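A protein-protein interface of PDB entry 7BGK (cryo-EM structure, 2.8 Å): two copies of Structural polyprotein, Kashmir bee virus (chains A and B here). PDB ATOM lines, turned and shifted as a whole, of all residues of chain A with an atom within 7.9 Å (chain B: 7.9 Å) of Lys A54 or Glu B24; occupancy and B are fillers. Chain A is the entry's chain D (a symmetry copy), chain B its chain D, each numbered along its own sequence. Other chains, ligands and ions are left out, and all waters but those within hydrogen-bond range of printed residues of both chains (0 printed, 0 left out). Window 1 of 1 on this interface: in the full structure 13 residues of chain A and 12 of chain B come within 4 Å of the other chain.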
ATOM      1  N   LYS A  47      35.203  -5.244  -9.643  1.00  0.00           N
ATOM      2  CA  LYS A  47      35.021  -3.794  -9.704  1.00  0.00           C
ATOM      3  C   LYS A  47      35.997  -3.252 -10.732  1.00  0.00           C
ATOM      4  O   LYS A  47      36.926  -2.502 -10.410  1.00  0.00           O
ATOM      5  CB  LYS A  47      35.210  -3.147  -8.334  1.00  0.00           C
ATOM      6  CG  LYS A  47      33.966  -3.207  -7.478  1.00  0.00           C
ATOM      7  CD  LYS A  47      33.903  -2.089  -6.469  1.00  0.00           C
ATOM      8  CE  LYS A  47      35.049  -2.151  -5.498  1.00  0.00           C
ATOM      9  NZ  LYS A  47      35.030  -1.000  -4.562  1.00  0.00           N
ATOM     10  N   THR A  50      34.593   0.373 -15.081  1.00  0.00           N
ATOM     11  CA  THR A  50      33.387   0.265 -15.878  1.00  0.00           C
ATOM     12  C   THR A  50      32.264   0.923 -15.091  1.00  0.00           C
ATOM     13  O   THR A  50      32.497   1.573 -14.069  1.00  0.00           O
ATOM     14  CB  THR A  50      33.016  -1.201 -16.135  1.00  0.00           C
ATOM     15  OG1 THR A  50      32.945  -1.888 -14.884  1.00  0.00           O
ATOM     16  CG2 THR A  50      34.050  -1.898 -16.978  1.00  0.00           C
ATOM     17  N   ALA A  51      31.036   0.722 -15.546  1.00  0.00           N
ATOM     18  CA  ALA A  51      29.861   1.201 -14.842  1.00  0.00           C
ATOM     19  C   ALA A  51      29.477   0.313 -13.671  1.00  0.00           C
ATOM     20  O   ALA A  51      28.350   0.416 -13.173  1.00  0.00           O
ATOM     21  CB  ALA A  51      28.691   1.332 -15.813  1.00  0.00           C
ATOM     22  N   ALA A  52      30.377  -0.566 -13.228  1.00  0.00           N
ATOM     23  CA  ALA A  52      30.124  -1.326 -12.012  1.00  0.00           C
ATOM     24  C   ALA A  52      30.208  -0.445 -10.774  1.00  0.00           C
ATOM     25  O   ALA A  52      29.428  -0.617  -9.832  1.00  0.00           O
ATOM     26  CB  ALA A  52      31.110  -2.483 -11.908  1.00  0.00           C
ATOM     27  N   VAL A  53      31.153   0.491 -10.744  1.00  0.00           N
ATOM     28  CA  VAL A  53      31.207   1.462  -9.661  1.00  0.00           C
ATOM     29  C   VAL A  53      30.206   2.568  -9.953  1.00  0.00           C
ATOM     30  O   VAL A  53      29.954   2.918 -11.111  1.00  0.00           O
ATOM     31  CB  VAL A  53      32.631   2.018  -9.466  1.00  0.00           C
ATOM     32  CG1 VAL A  53      33.595   0.906  -9.159  1.00  0.00           C
ATOM     33  CG2 VAL A  53      33.080   2.768 -10.669  1.00  0.00           C
ATOM     34  N   LYS A  54      29.628   3.128  -8.894  1.00  0.00           N
ATOM     35  CA  LYS A  54      28.527   4.067  -9.068  1.00  0.00           C
ATOM     36  C   LYS A  54      28.992   5.355  -9.732  1.00  0.00           C
ATOM     37  O   LYS A  54      28.400   5.800 -10.719  1.00  0.00           O
ATOM     38  CB  LYS A  54      27.882   4.349  -7.714  1.00  0.00           C
ATOM     39  CG  LYS A  54      26.809   5.417  -7.707  1.00  0.00           C
ATOM     40  CD  LYS A  54      25.572   4.982  -8.423  1.00  0.00           C
ATOM     41  CE  LYS A  54      24.685   6.160  -8.734  1.00  0.00           C
ATOM     42  NZ  LYS A  54      24.163   6.782  -7.503  1.00  0.00           N
ATOM     43  N   TRP A  55      30.035   5.986  -9.192  1.00  0.00           N
ATOM     44  CA  TRP A  55      30.441   7.294  -9.693  1.00  0.00           C
ATOM     45  C   TRP A  55      30.935   7.227 -11.135  1.00  0.00           C
ATOM     46  O   TRP A  55      30.634   8.115 -11.946  1.00  0.00           O
ATOM     47  CB  TRP A  55      31.502   7.895  -8.776  1.00  0.00           C
ATOM     48  CG  TRP A  55      32.751   7.114  -8.650  1.00  0.00           C
ATOM     49  CD1 TRP A  55      33.027   6.161  -7.728  1.00  0.00           C
ATOM     50  CD2 TRP A  55      33.913   7.233  -9.468  1.00  0.00           C
ATOM     51  NE1 TRP A  55      34.289   5.670  -7.922  1.00  0.00           N
ATOM     52  CE2 TRP A  55      34.853   6.311  -8.989  1.00  0.00           C
ATOM     53  CE3 TRP A  55      34.248   8.025 -10.567  1.00  0.00           C
ATOM     54  CZ2 TRP A  55      36.101   6.164  -9.563  1.00  0.00           C
ATOM     55  CZ3 TRP A  55      35.482   7.873 -11.133  1.00  0.00           C
ATOM     56  CH2 TRP A  55      36.396   6.951 -10.633  1.00  0.00           C
ATOM     57  N   PHE A  56      31.697   6.192 -11.480  1.00  0.00           N
ATOM     58  CA  PHE A  56      32.152   6.064 -12.856  1.00  0.00           C
ATOM     59  C   PHE A  56      30.978   5.840 -13.793  1.00  0.00           C
ATOM     60  O   PHE A  56      30.965   6.347 -14.918  1.00  0.00           O
ATOM     61  CB  PHE A  56      33.164   4.932 -12.984  1.00  0.00           C
ATOM     62  CG  PHE A  56      33.921   4.951 -14.273  1.00  0.00           C
ATOM     63  CD1 PHE A  56      34.863   5.924 -14.514  1.00  0.00           C
ATOM     64  CD2 PHE A  56      33.676   4.012 -15.251  1.00  0.00           C
ATOM     65  CE1 PHE A  56      35.548   5.954 -15.693  1.00  0.00           C
ATOM     66  CE2 PHE A  56      34.364   4.041 -16.434  1.00  0.00           C
ATOM     67  CZ  PHE A  56      35.299   5.009 -16.654  1.00  0.00           C
ATOM     68  N   ALA A  57      30.005   5.043 -13.361  1.00  0.00           N
ATOM     69  CA  ALA A  57      28.772   4.899 -14.121  1.00  0.00           C
ATOM     70  C   ALA A  57      28.089   6.240 -14.328  1.00  0.00           C
ATOM     71  O   ALA A  57      27.588   6.533 -15.420  1.00  0.00           O
ATOM     72  CB  ALA A  57      27.840   3.936 -13.398  1.00  0.00           C
ATOM     73  N   ASP A  58      28.044   7.062 -13.282  1.00  0.00           N
ATOM     74  CA  ASP A  58      27.453   8.388 -13.396  1.00  0.00           C
ATOM     75  C   ASP A  58      28.181   9.253 -14.410  1.00  0.00           C
ATOM     76  O   ASP A  58      27.558  10.069 -15.095  1.00  0.00           O
ATOM     77  CB  ASP A  58      27.478   9.066 -12.031  1.00  0.00           C
ATOM     78  CG  ASP A  58      26.640   8.343 -11.009  1.00  0.00           C
ATOM     79  OD1 ASP A  58      26.698   8.721  -9.819  1.00  0.00           O
ATOM     80  OD2 ASP A  58      25.922   7.402 -11.391  1.00  0.00           O
ATOM     81  N   ILE A  59      29.495   9.096 -14.508  1.00  0.00           N
ATOM     82  CA  ILE A  59      30.271   9.875 -15.468  1.00  0.00           C
ATOM     83  C   ILE A  59      30.060   9.369 -16.893  1.00  0.00           C
ATOM     84  O   ILE A  59      29.858  10.157 -17.824  1.00  0.00           O
ATOM     85  CB  ILE A  59      31.751   9.868 -15.059  1.00  0.00           C
ATOM     86  CG1 ILE A  59      31.881  10.622 -13.740  1.00  0.00           C
ATOM     87  CG2 ILE A  59      32.599  10.536 -16.106  1.00  0.00           C
ATOM     88  CD1 ILE A  59      33.207  10.605 -13.150  1.00  0.00           C
ATOM     89  N   VAL A  60      30.107   8.050 -17.086  1.00  0.00           N
ATOM     90  CA  VAL A  60      29.921   7.480 -18.422  1.00  0.00           C
ATOM     91  C   VAL A  60      28.504   7.710 -18.924  1.00  0.00           C
ATOM     92  O   VAL A  60      28.278   7.811 -20.134  1.00  0.00           O
ATOM     93  CB  VAL A  60      30.276   5.983 -18.444  1.00  0.00           C
ATOM     94  CG1 VAL A  60      31.695   5.742 -18.001  1.00  0.00           C
ATOM     95  CG2 VAL A  60      29.267   5.146 -17.696  1.00  0.00           C
ATOM     96  N   GLY A  61      27.539   7.801 -18.023  1.00  0.00           N
ATOM     97  CA  GLY A  61      26.188   8.155 -18.381  1.00  0.00           C
ATOM     98  C   GLY A  61      25.928   9.634 -18.374  1.00  0.00           C
ATOM     99  O   GLY A  61      24.825  10.069 -18.713  1.00  0.00           O
ATOM    100  N   VAL A  63      25.337  11.797 -15.950  1.00  0.00           N
ATOM    101  CA  VAL A  63      24.131  12.160 -15.227  1.00  0.00           C
ATOM    102  C   VAL A  63      24.204  13.628 -14.830  1.00  0.00           C
ATOM    103  O   VAL A  63      25.261  14.264 -14.853  1.00  0.00           O
ATOM    104  CB  VAL A  63      23.910  11.259 -14.002  1.00  0.00           C
ATOM    105  CG1 VAL A  63      23.717   9.834 -14.426  1.00  0.00           C
ATOM    106  CG2 VAL A  63      25.061  11.361 -13.051  1.00  0.00           C
ATOM    107  N   ALA A  64      23.049  14.179 -14.476  1.00  0.00           N
ATOM    108  CA  ALA A  64      22.952  15.607 -14.234  1.00  0.00           C
ATOM    109  C   ALA A  64      23.582  16.021 -12.917  1.00  0.00           C
ATOM    110  O   ALA A  64      23.846  17.210 -12.720  1.00  0.00           O
ATOM    111  CB  ALA A  64      21.491  16.035 -14.263  1.00  0.00           C
ATOM    112  N   ALA A  65      23.828  15.077 -12.014  1.00  0.00           N
ATOM    113  CA  ALA A  65      24.339  15.428 -10.699  1.00  0.00           C
ATOM    114  C   ALA A  65      25.811  15.802 -10.765  1.00  0.00           C
ATOM    115  O   ALA A  65      26.263  16.687 -10.032  1.00  0.00           O
ATOM    116  CB  ALA A  65      24.128  14.273  -9.732  1.00  0.00           C
ATOM    117  N   ILE A  66      26.575  15.142 -11.635  1.00  0.00           N
ATOM    118  CA  ILE A  66      27.993  15.438 -11.758  1.00  0.00           C
ATOM    119  C   ILE A  66      28.235  16.827 -12.317  1.00  0.00           C
ATOM    120  O   ILE A  66      29.379  17.289 -12.337  1.00  0.00           O
ATOM    121  CB  ILE A  66      28.699  14.382 -12.631  1.00  0.00           C
ATOM    122  CG1 ILE A  66      28.086  14.314 -14.018  1.00  0.00           C
ATOM    123  CG2 ILE A  66      28.589  13.035 -12.000  1.00  0.00           C
ATOM    124  CD1 ILE A  66      29.007  13.783 -15.054  1.00  0.00           C
ATOM    125  N   PRO B  12      25.080  -1.167 -10.873  1.00  0.00           N
ATOM    126  CA  PRO B  12      26.261  -0.903 -10.059  1.00  0.00           C
ATOM    127  C   PRO B  12      26.348  -1.820  -8.853  1.00  0.00           C
ATOM    128  O   PRO B  12      25.319  -2.236  -8.322  1.00  0.00           O
ATOM    129  CB  PRO B  12      26.057   0.549  -9.644  1.00  0.00           C
ATOM    130  CG  PRO B  12      25.440   1.156 -10.818  1.00  0.00           C
ATOM    131  CD  PRO B  12      24.549   0.082 -11.441  1.00  0.00           C
ATOM    132  N   THR B  13      27.566  -2.121  -8.415  1.00  0.00           N
ATOM    133  CA  THR B  13      27.802  -3.114  -7.372  1.00  0.00           C
ATOM    134  C   THR B  13      27.918  -2.409  -6.028  1.00  0.00           C
ATOM    135  O   THR B  13      28.929  -1.776  -5.725  1.00  0.00           O
ATOM    136  CB  THR B  13      29.035  -3.973  -7.649  1.00  0.00           C
ATOM    137  OG1 THR B  13      30.215  -3.171  -7.784  1.00  0.00           O
ATOM    138  CG2 THR B  13      28.814  -4.901  -8.830  1.00  0.00           C
ATOM    139  N   SER B  14      26.864  -2.526  -5.232  1.00  0.00           N
ATOM    140  CA  SER B  14      26.732  -1.926  -3.922  1.00  0.00           C
ATOM    141  C   SER B  14      26.535  -3.073  -2.943  1.00  0.00           C
ATOM    142  O   SER B  14      26.167  -4.185  -3.330  1.00  0.00           O
ATOM    143  CB  SER B  14      25.547  -0.955  -3.862  1.00  0.00           C
ATOM    144  OG  SER B  14      25.324  -0.356  -2.592  1.00  0.00           O
ATOM    145  N   LYS B  18      20.096   0.640  -1.081  1.00  0.00           N
ATOM    146  CA  LYS B  18      19.922   1.866  -1.844  1.00  0.00           C
ATOM    147  C   LYS B  18      21.270   2.149  -2.485  1.00  0.00           C
ATOM    148  O   LYS B  18      22.249   2.399  -1.775  1.00  0.00           O
ATOM    149  CB  LYS B  18      19.479   2.991  -0.910  1.00  0.00           C
ATOM    150  CG  LYS B  18      19.178   4.306  -1.549  1.00  0.00           C
ATOM    151  CD  LYS B  18      18.705   5.302  -0.509  1.00  0.00           C
ATOM    152  CE  LYS B  18      18.412   6.651  -1.124  1.00  0.00           C
ATOM    153  NZ  LYS B  18      17.947   7.639  -0.118  1.00  0.00           N
ATOM    154  N   ILE B  19      21.336   2.117  -3.815  1.00  0.00           N
ATOM    155  CA  ILE B  19      22.662   2.129  -4.424  1.00  0.00           C
ATOM    156  C   ILE B  19      23.354   3.454  -4.142  1.00  0.00           C
ATOM    157  O   ILE B  19      24.541   3.500  -3.799  1.00  0.00           O
ATOM    158  CB  ILE B  19      22.580   1.861  -5.936  1.00  0.00           C
ATOM    159  CG1 ILE B  19      21.871   0.538  -6.242  1.00  0.00           C
ATOM    160  CG2 ILE B  19      23.973   1.795  -6.521  1.00  0.00           C
ATOM    161  CD1 ILE B  19      22.403  -0.765  -5.665  1.00  0.00           C
ATOM    162  N   GLY B  20      22.609   4.548  -4.266  1.00  0.00           N
ATOM    163  CA  GLY B  20      23.101   5.872  -4.002  1.00  0.00           C
ATOM    164  C   GLY B  20      22.089   6.761  -3.313  1.00  0.00           C
ATOM    165  O   GLY B  20      20.955   6.367  -3.039  1.00  0.00           O
ATOM    166  N   PRO B  21      22.488   7.996  -3.038  1.00  0.00           N
ATOM    167  CA  PRO B  21      21.714   8.860  -2.141  1.00  0.00           C
ATOM    168  C   PRO B  21      20.458   9.433  -2.783  1.00  0.00           C
ATOM    169  O   PRO B  21      19.417   9.585  -2.135  1.00  0.00           O
ATOM    170  CB  PRO B  21      22.715   9.977  -1.819  1.00  0.00           C
ATOM    171  CG  PRO B  21      24.025   9.463  -2.339  1.00  0.00           C
ATOM    172  CD  PRO B  21      23.642   8.747  -3.549  1.00  0.00           C
ATOM    173  N   ILE B  22      20.572   9.756  -4.069  1.00  0.00           N
ATOM    174  CA  ILE B  22      19.535  10.412  -4.849  1.00  0.00           C
ATOM    175  C   ILE B  22      19.200   9.590  -6.080  1.00  0.00           C
ATOM    176  O   ILE B  22      19.913   8.660  -6.459  1.00  0.00           O
ATOM    177  CB  ILE B  22      19.938  11.828  -5.284  1.00  0.00           C
ATOM    178  CG1 ILE B  22      21.180  11.766  -6.161  1.00  0.00           C
ATOM    179  CG2 ILE B  22      20.192  12.666  -4.082  1.00  0.00           C
ATOM    180  CD1 ILE B  22      21.510  13.044  -6.800  1.00  0.00           C
ATOM    181  N   SER B  23      18.082   9.955  -6.700  1.00  0.00           N
ATOM    182  CA  SER B  23      17.703   9.405  -7.987  1.00  0.00           C
ATOM    183  C   SER B  23      18.417  10.151  -9.098  1.00  0.00           C
ATOM    184  O   SER B  23      18.340  11.377  -9.186  1.00  0.00           O
ATOM    185  CB  SER B  23      16.195   9.530  -8.180  1.00  0.00           C
ATOM    186  OG  SER B  23      15.324   8.813  -7.345  1.00  0.00           O
ATOM    187  N   GLU B  24      19.110   9.404  -9.944  1.00  0.00           N
ATOM    188  CA  GLU B  24      19.909   9.994 -10.998  1.00  0.00           C
ATOM    189  C   GLU B  24      19.027  10.251 -12.209  1.00  0.00           C
ATOM    190  O   GLU B  24      18.256   9.381 -12.620  1.00  0.00           O
ATOM    191  CB  GLU B  24      21.095   9.105 -11.367  1.00  0.00           C
ATOM    192  CG  GLU B  24      21.746   8.393 -10.197  1.00  0.00           C
ATOM    193  CD  GLU B  24      22.583   9.327  -9.343  1.00  0.00           C
ATOM    194  OE1 GLU B  24      22.983  10.397  -9.844  1.00  0.00           O
ATOM    195  OE2 GLU B  24      22.847   8.991  -8.171  1.00  0.00           O
ATOM    196  N   VAL B  25      19.103  11.483 -12.718  1.00  0.00           N
ATOM    197  CA  VAL B  25      18.343  11.843 -13.948  1.00  0.00           C
ATOM    198  C   VAL B  25      19.361  11.879 -15.086  1.00  0.00           C
ATOM    199  O   VAL B  25      20.437  12.479 -14.890  1.00  0.00           O
ATOM    200  CB  VAL B  25      17.621  13.194 -13.795  1.00  0.00           C
ATOM    201  CG1 VAL B  25      16.945  13.620 -15.089  1.00  0.00           C
ATOM    202  CG2 VAL B  25      16.621  13.177 -12.647  1.00  0.00           C
ATOM    203  N   ALA B  26      19.041  11.253 -16.220  1.00  0.00           N
ATOM    204  CA  ALA B  26      19.947  11.214 -17.350  1.00  0.00           C
ATOM    205  C   ALA B  26      20.073  12.589 -17.999  1.00  0.00           C
ATOM    206  O   ALA B  26      19.360  13.541 -17.675  1.00  0.00           O
ATOM    207  CB  ALA B  26      19.477  10.180 -18.365  1.00  0.00           C
ATOM    208  N   SER B  27      21.018  12.673 -18.938  1.00  0.00           N
ATOM    209  CA  SER B  27      21.445  13.950 -19.505  1.00  0.00           C
ATOM    210  C   SER B  27      21.232  14.059 -21.011  1.00  0.00           C
ATOM    211  O   SER B  27      20.446  14.907 -21.438  1.00  0.00           O
ATOM    212  CB  SER B  27      22.894  14.214 -19.113  1.00  0.00           C
ATOM    213  OG  SER B  27      23.814  13.352 -19.745  1.00  0.00           O
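N of Thr B13 lies within hydrogen-bond range of O of Ala A52, 2.8 Å away. NZ of Lys A54 is in salt-bridge range of OE2 of Glu B24, 2.7 Å away. N of Ala A64 lies within hydrogen-bond range of O of Val B25 (3.1 Å).
Among the printed residues, merely in contact across the chains: Ala A52 with Pro B12 (3.2 Å), Gly A61 with Ser B27 (3.6 Å), Val A63 with Val B25 (3.7 Å), Lys A47 with Thr B13 (3.8 Å), Lys A54 with Gly B20 (3.8 Å), Ala A51 with Pro B12 (3.8 Å) and Val A63 with Glu B24 (3.9 Å).
Printed residues of chain B within 4 Å of Lys A54: Gly B20 (3.8 Å) and Glu B24 (2.7 Å). Of chain A, only Lys A54 and Val A63 come within 4 Å of Glu B24. Printed residues of chain B within 4 Å of Gly A61: Ser B27 (3.6 Å). Printed residues of chain B within 4 Å of Ala A64: Val B25 (3.1 Å). Printed residues of chain A within 4 Å of Pro B12: Ala A51 (3.8 Å) and Ala A52 (3.2 Å). Of the printed residues of chain B, Val A63 touches Glu B24 and Val B25. Of the printed residues of chain A, Val B25 touches Val A63 (3.7 Å) and Ala A64 (3.1 Å). Asp A58 touches none of the printed residues of chain B. The nearest residue of chain A that does not touch Glu B24 is Ala A65 (4.04 Å). The nearest printed residue of chain A that does not touch Ser B27 is Val A63 (4.4 Å).
The side-chain hydroxyl (OG1) of Thr A50 sits close to the backbone NH (N) of Ala A52. The side-chain amino group of Lys A54 is in salt-bridge range of the side-chain carboxylate of Asp A58, 3.9 Å away. The backbone carbonyl oxygen (O) of Asp A58 sits at hydrogen-bond distance from the backbone NH (N) of Val A63 (2.9 Å).
No position is printed for both chains.
Of the 13 printed residues of chain B, 6 touch a printed residue of chain A. Printed residues of chain B that touch a printed residue of chain A: Pro B12, Thr B13, Gly B20, Glu B24, Val B25 and Ser B27. Of the 17 printed residues of chain A, 7 touch a printed residue of chain B. Printed residues of chain A that touch a printed residue of chain B: Lys A47, Ala A51, Ala A52, Lys A54, Gly A61, Val A63 and Ala A64. Hydrophobic or aromatic side chains of chain A within 4 Å of the printed part of chain B: Val A63 and Ala A64. Among the printed residues, 10 pairs touch across the chains. Among the printed residues, Asp or Glu carboxylates within 4 Å of a Lys or Arg side-chain nitrogen of the other chain: Lys A54 with Glu B24.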
